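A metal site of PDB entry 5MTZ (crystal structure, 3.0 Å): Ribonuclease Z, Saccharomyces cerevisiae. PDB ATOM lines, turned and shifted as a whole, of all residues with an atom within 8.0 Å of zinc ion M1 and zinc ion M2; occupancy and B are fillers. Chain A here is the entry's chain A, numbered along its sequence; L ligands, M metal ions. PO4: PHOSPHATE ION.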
ATOM      1  N   GLY A 510       1.670   9.151 -29.008  1.00  0.00           N
ATOM      2  CA  GLY A 510       1.042  10.112 -29.912  1.00  0.00           C
ATOM      3  C   GLY A 510      -0.009  11.039 -29.323  1.00  0.00           C
ATOM      4  O   GLY A 510      -0.570  10.783 -28.256  1.00  0.00           O
ATOM      5  N   SER A 511      -0.279  12.098 -30.063  1.00  0.00           N
ATOM      6  CA  SER A 511      -1.220  13.140 -29.643  1.00  0.00           C
ATOM      7  C   SER A 511      -2.596  12.938 -30.256  1.00  0.00           C
ATOM      8  O   SER A 511      -2.705  12.684 -31.444  1.00  0.00           O
ATOM      9  CB  SER A 511      -0.691  14.528 -30.041  1.00  0.00           C
ATOM     10  OG  SER A 511      -1.616  15.550 -29.673  1.00  0.00           O
ATOM     11  N   ALA A 512      -3.630  13.070 -29.431  1.00  0.00           N
ATOM     12  CA  ALA A 512      -5.015  13.246 -29.899  1.00  0.00           C
ATOM     13  C   ALA A 512      -5.573  12.111 -30.777  1.00  0.00           C
ATOM     14  O   ALA A 512      -6.332  11.273 -30.296  1.00  0.00           O
ATOM     15  CB  ALA A 512      -5.151  14.593 -30.604  1.00  0.00           C
ATOM     16  N   LEU A 513      -5.194  12.110 -32.050  1.00  0.00           N
ATOM     17  CA  LEU A 513      -5.683  11.141 -33.054  1.00  0.00           C
ATOM     18  C   LEU A 513      -4.725   9.966 -33.075  1.00  0.00           C
ATOM     19  O   LEU A 513      -3.515  10.183 -33.039  1.00  0.00           O
ATOM     20  CB  LEU A 513      -5.768  11.829 -34.442  1.00  0.00           C
ATOM     21  CG  LEU A 513      -5.602  11.050 -35.775  1.00  0.00           C
ATOM     22  CD1 LEU A 513      -6.533  11.607 -36.852  1.00  0.00           C
ATOM     23  CD2 LEU A 513      -4.156  11.003 -36.304  1.00  0.00           C
ATOM     24  N   VAL A 520      -2.354   6.465 -29.812  1.00  0.00           N
ATOM     25  CA  VAL A 520      -2.566   7.226 -28.587  1.00  0.00           C
ATOM     26  C   VAL A 520      -1.826   6.700 -27.333  1.00  0.00           C
ATOM     27  O   VAL A 520      -1.591   5.482 -27.169  1.00  0.00           O
ATOM     28  CB  VAL A 520      -4.066   7.402 -28.256  1.00  0.00           C
ATOM     29  CG1 VAL A 520      -4.746   8.260 -29.303  1.00  0.00           C
ATOM     30  CG2 VAL A 520      -4.768   6.057 -28.087  1.00  0.00           C
ATOM     31  N   VAL A 521      -1.553   7.638 -26.433  1.00  0.00           N
ATOM     32  CA  VAL A 521      -0.580   7.487 -25.332  1.00  0.00           C
ATOM     33  C   VAL A 521      -0.858   6.318 -24.401  1.00  0.00           C
ATOM     34  O   VAL A 521      -2.007   6.036 -24.054  1.00  0.00           O
ATOM     35  CB  VAL A 521      -0.497   8.687 -24.355  1.00  0.00           C
ATOM     36  CG1 VAL A 521       0.927   8.873 -23.837  1.00  0.00           C
ATOM     37  CG2 VAL A 521      -0.999   9.998 -24.959  1.00  0.00           C
ATOM     38  N   ASP A 544      -1.745   6.625 -17.925  1.00  0.00           N
ATOM     39  CA  ASP A 544      -2.669   6.733 -19.060  1.00  0.00           C
ATOM     40  C   ASP A 544      -2.710   5.439 -19.902  1.00  0.00           C
ATOM     41  O   ASP A 544      -1.861   4.538 -19.761  1.00  0.00           O
ATOM     42  CB  ASP A 544      -2.391   7.971 -19.943  1.00  0.00           C
ATOM     43  CG  ASP A 544      -2.336   9.268 -19.129  1.00  0.00           C
ATOM     44  OD1 ASP A 544      -2.557   9.187 -17.904  1.00  0.00           O
ATOM     45  OD2 ASP A 544      -2.065  10.357 -19.695  1.00  0.00           O
ATOM     46  N   SER A 575      -4.002  11.202 -16.137  1.00  0.00           N
ATOM     47  CA  SER A 575      -3.609  12.601 -16.002  1.00  0.00           C
ATOM     48  C   SER A 575      -4.824  13.537 -16.105  1.00  0.00           C
ATOM     49  O   SER A 575      -4.987  14.403 -15.259  1.00  0.00           O
ATOM     50  CB  SER A 575      -2.572  12.962 -17.051  1.00  0.00           C
ATOM     51  OG  SER A 575      -3.142  13.066 -18.353  1.00  0.00           O
ATOM     52  N   HIS A 576      -5.643  13.375 -17.129  1.00  0.00           N
ATOM     53  CA  HIS A 576      -6.829  14.219 -17.314  1.00  0.00           C
ATOM     54  C   HIS A 576      -7.892  13.561 -18.192  1.00  0.00           C
ATOM     55  O   HIS A 576      -7.708  12.444 -18.674  1.00  0.00           O
ATOM     56  CB  HIS A 576      -6.425  15.582 -17.866  1.00  0.00           C
ATOM     57  CG  HIS A 576      -5.822  15.542 -19.229  1.00  0.00           C
ATOM     58  ND1 HIS A 576      -4.710  14.783 -19.510  1.00  0.00           N
ATOM     59  CD2 HIS A 576      -6.155  16.177 -20.375  1.00  0.00           C
ATOM     60  CE1 HIS A 576      -4.383  14.949 -20.784  1.00  0.00           C
ATOM     61  NE2 HIS A 576      -5.238  15.792 -21.333  1.00  0.00           N
ATOM     62  N   LEU A 577      -9.007  14.260 -18.393  1.00  0.00           N
ATOM     63  CA  LEU A 577     -10.182  13.662 -19.023  1.00  0.00           C
ATOM     64  C   LEU A 577     -10.210  13.639 -20.557  1.00  0.00           C
ATOM     65  O   LEU A 577     -11.210  13.224 -21.149  1.00  0.00           O
ATOM     66  CB  LEU A 577     -11.456  14.340 -18.495  1.00  0.00           C
ATOM     67  CG  LEU A 577     -11.579  14.220 -16.979  1.00  0.00           C
ATOM     68  CD1 LEU A 577     -12.521  15.298 -16.465  1.00  0.00           C
ATOM     69  CD2 LEU A 577     -12.031  12.825 -16.557  1.00  0.00           C
ATOM     70  N   HIS A 578      -9.131  14.044 -21.224  1.00  0.00           N
ATOM     71  CA  HIS A 578      -9.117  13.967 -22.666  1.00  0.00           C
ATOM     72  C   HIS A 578      -9.104  12.507 -23.094  1.00  0.00           C
ATOM     73  O   HIS A 578      -8.402  11.674 -22.507  1.00  0.00           O
ATOM     74  CB  HIS A 578      -7.950  14.738 -23.269  1.00  0.00           C
ATOM     75  CG  HIS A 578      -8.150  16.220 -23.287  1.00  0.00           C
ATOM     76  ND1 HIS A 578      -7.110  17.112 -23.457  1.00  0.00           N
ATOM     77  CD2 HIS A 578      -9.263  16.968 -23.137  1.00  0.00           C
ATOM     78  CE1 HIS A 578      -7.588  18.344 -23.429  1.00  0.00           C
ATOM     79  NE2 HIS A 578      -8.895  18.280 -23.223  1.00  0.00           N
ATOM     80  N   ALA A 579      -9.919  12.220 -24.107  1.00  0.00           N
ATOM     81  CA  ALA A 579     -10.167  10.835 -24.570  1.00  0.00           C
ATOM     82  C   ALA A 579      -8.902  10.095 -25.085  1.00  0.00           C
ATOM     83  O   ALA A 579      -8.848   8.860 -24.987  1.00  0.00           O
ATOM     84  CB  ALA A 579     -11.277  10.842 -25.631  1.00  0.00           C
ATOM     85  N   ASP A 580      -7.896  10.849 -25.569  1.00  0.00           N
ATOM     86  CA  ASP A 580      -6.626  10.241 -26.000  1.00  0.00           C
ATOM     87  C   ASP A 580      -5.818   9.644 -24.859  1.00  0.00           C
ATOM     88  O   ASP A 580      -4.859   8.926 -25.124  1.00  0.00           O
ATOM     89  CB  ASP A 580      -5.722  11.186 -26.847  1.00  0.00           C
ATOM     90  CG  ASP A 580      -5.336  12.459 -26.110  1.00  0.00           C
ATOM     91  OD1 ASP A 580      -6.268  13.076 -25.573  1.00  0.00           O
ATOM     92  OD2 ASP A 580      -4.133  12.873 -26.072  1.00  0.00           O
ATOM     93  N   HIS A 581      -6.213   9.905 -23.607  1.00  0.00           N
ATOM     94  CA  HIS A 581      -5.506   9.356 -22.444  1.00  0.00           C
ATOM     95  C   HIS A 581      -6.195   8.242 -21.674  1.00  0.00           C
ATOM     96  O   HIS A 581      -5.513   7.514 -20.955  1.00  0.00           O
ATOM     97  CB  HIS A 581      -5.092  10.461 -21.483  1.00  0.00           C
ATOM     98  CG  HIS A 581      -4.176  11.458 -22.109  1.00  0.00           C
ATOM     99  ND1 HIS A 581      -2.812  11.453 -21.923  1.00  0.00           N
ATOM    100  CD2 HIS A 581      -4.427  12.443 -23.003  1.00  0.00           C
ATOM    101  CE1 HIS A 581      -2.268  12.416 -22.637  1.00  0.00           C
ATOM    102  NE2 HIS A 581      -3.232  13.028 -23.315  1.00  0.00           N
ATOM    103  N   HIS A 706      -3.498  23.114 -18.686  1.00  0.00           N
ATOM    104  CA  HIS A 706      -4.034  22.467 -19.868  1.00  0.00           C
ATOM    105  C   HIS A 706      -5.555  22.555 -19.831  1.00  0.00           C
ATOM    106  O   HIS A 706      -6.149  23.507 -20.361  1.00  0.00           O
ATOM    107  CB  HIS A 706      -3.504  21.022 -19.944  1.00  0.00           C
ATOM    108  CG  HIS A 706      -3.966  20.234 -21.125  1.00  0.00           C
ATOM    109  ND1 HIS A 706      -3.777  20.650 -22.425  1.00  0.00           N
ATOM    110  CD2 HIS A 706      -4.595  19.031 -21.204  1.00  0.00           C
ATOM    111  CE1 HIS A 706      -4.272  19.751 -23.259  1.00  0.00           C
ATOM    112  NE2 HIS A 706      -4.759  18.746 -22.549  1.00  0.00           N
ATOM    113  N   CYS A 707      -6.155  21.603 -19.140  1.00  0.00           N
ATOM    114  CA  CYS A 707      -7.597  21.439 -19.071  1.00  0.00           C
ATOM    115  C   CYS A 707      -7.930  21.839 -17.626  1.00  0.00           C
ATOM    116  O   CYS A 707      -7.023  21.937 -16.801  1.00  0.00           O
ATOM    117  CB  CYS A 707      -7.916  19.950 -19.376  1.00  0.00           C
ATOM    118  SG  CYS A 707      -9.632  19.408 -19.450  1.00  0.00           S
ATOM    119  N   ALA A 710      -6.869  18.865 -14.893  1.00  0.00           N
ATOM    120  CA  ALA A 710      -5.703  18.173 -15.410  1.00  0.00           C
ATOM    121  C   ALA A 710      -4.679  18.093 -14.295  1.00  0.00           C
ATOM    122  O   ALA A 710      -4.812  18.790 -13.273  1.00  0.00           O
ATOM    123  CB  ALA A 710      -5.144  18.892 -16.606  1.00  0.00           C
ATOM    124  N   TYR A 732       5.500  12.469 -14.168  1.00  0.00           N
ATOM    125  CA  TYR A 732       4.794  12.408 -15.454  1.00  0.00           C
ATOM    126  C   TYR A 732       3.902  13.593 -15.605  1.00  0.00           C
ATOM    127  O   TYR A 732       2.955  13.766 -14.862  1.00  0.00           O
ATOM    128  CB  TYR A 732       3.962  11.108 -15.579  1.00  0.00           C
ATOM    129  CG  TYR A 732       3.083  10.989 -16.835  1.00  0.00           C
ATOM    130  CD1 TYR A 732       3.564  11.312 -18.095  1.00  0.00           C
ATOM    131  CD2 TYR A 732       1.780  10.512 -16.746  1.00  0.00           C
ATOM    132  CE1 TYR A 732       2.769  11.201 -19.229  1.00  0.00           C
ATOM    133  CE2 TYR A 732       0.976  10.402 -17.884  1.00  0.00           C
ATOM    134  CZ  TYR A 732       1.480  10.742 -19.123  1.00  0.00           C
ATOM    135  OH  TYR A 732       0.708  10.635 -20.256  1.00  0.00           O
ATOM    136  N   GLY A 734       1.010  15.776 -17.469  1.00  0.00           N
ATOM    137  CA  GLY A 734      -0.204  15.482 -18.208  1.00  0.00           C
ATOM    138  C   GLY A 734       0.009  15.837 -19.666  1.00  0.00           C
ATOM    139  O   GLY A 734       0.889  15.291 -20.342  1.00  0.00           O
ATOM    140  N   ASP A 735      -0.840  16.748 -20.138  1.00  0.00           N
ATOM    141  CA  ASP A 735      -0.642  17.424 -21.397  1.00  0.00           C
ATOM    142  C   ASP A 735      -0.331  18.878 -20.990  1.00  0.00           C
ATOM    143  O   ASP A 735      -0.879  19.814 -21.566  1.00  0.00           O
ATOM    144  CB  ASP A 735      -1.924  17.346 -22.257  1.00  0.00           C
ATOM    145  CG  ASP A 735      -2.095  16.025 -23.044  1.00  0.00           C
ATOM    146  OD1 ASP A 735      -1.141  15.235 -23.038  1.00  0.00           O
ATOM    147  OD2 ASP A 735      -3.200  15.810 -23.660  1.00  0.00           O
ATOM    148  N   THR A 736       0.548  19.073 -20.016  1.00  0.00           N
ATOM    149  CA  THR A 736       0.739  20.413 -19.446  1.00  0.00           C
ATOM    150  C   THR A 736       1.480  21.335 -20.415  1.00  0.00           C
ATOM    151  O   THR A 736       2.270  20.910 -21.261  1.00  0.00           O
ATOM    152  CB  THR A 736       1.427  20.387 -18.041  1.00  0.00           C
ATOM    153  OG1 THR A 736       1.167  21.616 -17.340  1.00  0.00           O
ATOM    154  CG2 THR A 736       2.949  20.123 -18.133  1.00  0.00           C
ATOM    155  N   GLU A 757       5.616  15.296 -21.733  1.00  0.00           N
ATOM    156  CA  GLU A 757       4.908  15.526 -22.978  1.00  0.00           C
ATOM    157  C   GLU A 757       5.722  16.406 -23.894  1.00  0.00           C
ATOM    158  O   GLU A 757       6.187  17.466 -23.477  1.00  0.00           O
ATOM    159  CB  GLU A 757       3.577  16.189 -22.624  1.00  0.00           C
ATOM    160  CG  GLU A 757       2.702  16.609 -23.794  1.00  0.00           C
ATOM    161  CD  GLU A 757       2.697  18.087 -24.000  1.00  0.00           C
ATOM    162  OE1 GLU A 757       3.648  18.587 -24.609  1.00  0.00           O
ATOM    163  OE2 GLU A 757       1.726  18.750 -23.559  1.00  0.00           O
ATOM    164  N   THR A 759       4.577  17.332 -27.378  1.00  0.00           N
ATOM    165  CA  THR A 759       3.631  17.330 -28.496  1.00  0.00           C
ATOM    166  C   THR A 759       4.232  17.953 -29.734  1.00  0.00           C
ATOM    167  O   THR A 759       4.434  17.272 -30.736  1.00  0.00           O
ATOM    168  CB  THR A 759       2.294  18.052 -28.127  1.00  0.00           C
ATOM    169  OG1 THR A 759       1.777  17.524 -26.895  1.00  0.00           O
ATOM    170  CG2 THR A 759       1.237  17.839 -29.191  1.00  0.00           C
ATOM    171  N   LYS A 771      -2.902  25.536 -28.007  1.00  0.00           N
ATOM    172  CA  LYS A 771      -3.335  24.175 -27.707  1.00  0.00           C
ATOM    173  C   LYS A 771      -2.881  23.642 -26.332  1.00  0.00           C
ATOM    174  O   LYS A 771      -3.298  22.555 -25.940  1.00  0.00           O
ATOM    175  CB  LYS A 771      -2.864  23.225 -28.810  1.00  0.00           C
ATOM    176  CG  LYS A 771      -3.632  23.425 -30.115  1.00  0.00           C
ATOM    177  CD  LYS A 771      -3.118  22.482 -31.192  1.00  0.00           C
ATOM    178  CE  LYS A 771      -4.070  22.448 -32.367  1.00  0.00           C
ATOM    179  NZ  LYS A 771      -3.632  21.415 -33.344  1.00  0.00           N
ATOM    180  N   LYS A 772      -2.037  24.403 -25.638  1.00  0.00           N
ATOM    181  CA  LYS A 772      -1.594  24.138 -24.251  1.00  0.00           C
ATOM    182  C   LYS A 772      -0.783  22.849 -24.098  1.00  0.00           C
ATOM    183  O   LYS A 772      -1.032  22.044 -23.208  1.00  0.00           O
ATOM    184  CB  LYS A 772      -2.765  24.255 -23.244  1.00  0.00           C
ATOM    185  CG  LYS A 772      -2.989  25.690 -22.802  1.00  0.00           C
ATOM    186  CD  LYS A 772      -4.143  25.869 -21.828  1.00  0.00           C
ATOM    187  CE  LYS A 772      -5.465  26.066 -22.550  1.00  0.00           C
ATOM    188  NZ  LYS A 772      -6.615  26.051 -21.614  1.00  0.00           N
ATOM    189  N   HIS A 773       0.211  22.677 -24.978  1.00  0.00           N
ATOM    190  CA  HIS A 773       1.232  21.626 -24.875  1.00  0.00           C
ATOM    191  C   HIS A 773       2.618  22.244 -24.921  1.00  0.00           C
ATOM    192  O   HIS A 773       2.779  23.328 -25.473  1.00  0.00           O
ATOM    193  CB  HIS A 773       1.140  20.638 -26.043  1.00  0.00           C
ATOM    194  CG  HIS A 773      -0.160  19.895 -26.106  1.00  0.00           C
ATOM    195  ND1 HIS A 773      -0.365  18.715 -25.429  1.00  0.00           N
ATOM    196  CD2 HIS A 773      -1.312  20.173 -26.760  1.00  0.00           C
ATOM    197  CE1 HIS A 773      -1.594  18.290 -25.659  1.00  0.00           C
ATOM    198  NE2 HIS A 773      -2.187  19.157 -26.458  1.00  0.00           N
ATOM    199  N   HIS A 795       4.023  11.434 -26.311  1.00  0.00           N
ATOM    200  CA  HIS A 795       2.873  12.253 -26.679  1.00  0.00           C
ATOM    201  C   HIS A 795       3.280  13.224 -27.784  1.00  0.00           C
ATOM    202  O   HIS A 795       3.118  14.439 -27.650  1.00  0.00           O
ATOM    203  CB  HIS A 795       2.310  12.998 -25.471  1.00  0.00           C
ATOM    204  CG  HIS A 795       0.958  13.574 -25.698  1.00  0.00           C
ATOM    205  ND1 HIS A 795       0.727  14.581 -26.607  1.00  0.00           N
ATOM    206  CD2 HIS A 795      -0.240  13.283 -25.144  1.00  0.00           C
ATOM    207  CE1 HIS A 795      -0.561  14.881 -26.598  1.00  0.00           C
ATOM    208  NE2 HIS A 795      -1.172  14.101 -25.722  1.00  0.00           N
HETATM  209  P   PO4 L   1      -4.699  16.576 -26.567  1.00  0.00           P
HETATM  210  O1  PO4 L   1      -4.901  17.342 -25.271  1.00  0.00           O
HETATM  211  O2  PO4 L   1      -3.456  15.710 -26.537  1.00  0.00           O
HETATM  212  O3  PO4 L   1      -4.656  17.545 -27.727  1.00  0.00           O
HETATM  213  O4  PO4 L   1      -5.867  15.662 -26.763  1.00  0.00           O
HETATM  214 ZN    ZN M   1      -5.094  16.629 -23.407  1.00  0.00          ZN
HETATM  215 ZN    ZN M   2      -3.089  14.356 -25.118  1.00  0.00          ZN
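Zinc ion M2 is bound by an oxygen (O2) of the ligand (2.0 Å), a ring nitrogen (NE2) of His 795 (2.0 Å), the side-chain carboxylate (OD2) of Asp 580 (2.0 Å), the side-chain carboxylate (OD2) of Asp 735 (2.1 Å) and a ring nitrogen (NE2) of His 581 (2.2 Å).
Zinc ion M1 is bound by an oxygen (O1) of the ligand (2.0 Å), a ring nitrogen (ND1) of His 578 (2.1 Å), the side-chain carboxylate (OD2) of Asp 735 (2.1 Å), a ring nitrogen (NE2) of His 576 (2.2 Å) and a ring nitrogen (NE2) of His 706 (2.3 Å). Zinc ion M1 has five donor atoms within binding distance.
Within 4 Å of zinc ion M2: Asp 580, His 581, Asp 735 and His 795. Along chain A the residues within 4 Å of zinc ion M2 span positions 580 to 795. The nearest printed residue that does not touch zinc ion M2 is His 773 (4.2 Å).
ND1 of His 795 is in hydrogen-bond range of OG1 of Thr 759. The side-chain carboxylate (OD2) of Asp 580 sits close to the backbone NH (N) of Ala 512. The side-chain hydroxyl (OG) of Ser 575 sits at hydrogen-bond distance from a ring nitrogen (ND1) of His 576. ND1 of His 581 is in hydrogen-bond range of OD2 of Asp 544, 2.6 Å away. The backbone carbonyl oxygen (O) of His 706 lies within hydrogen-bond range of the side-chain amino group (NZ) of Lys 772 (2.9 Å).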
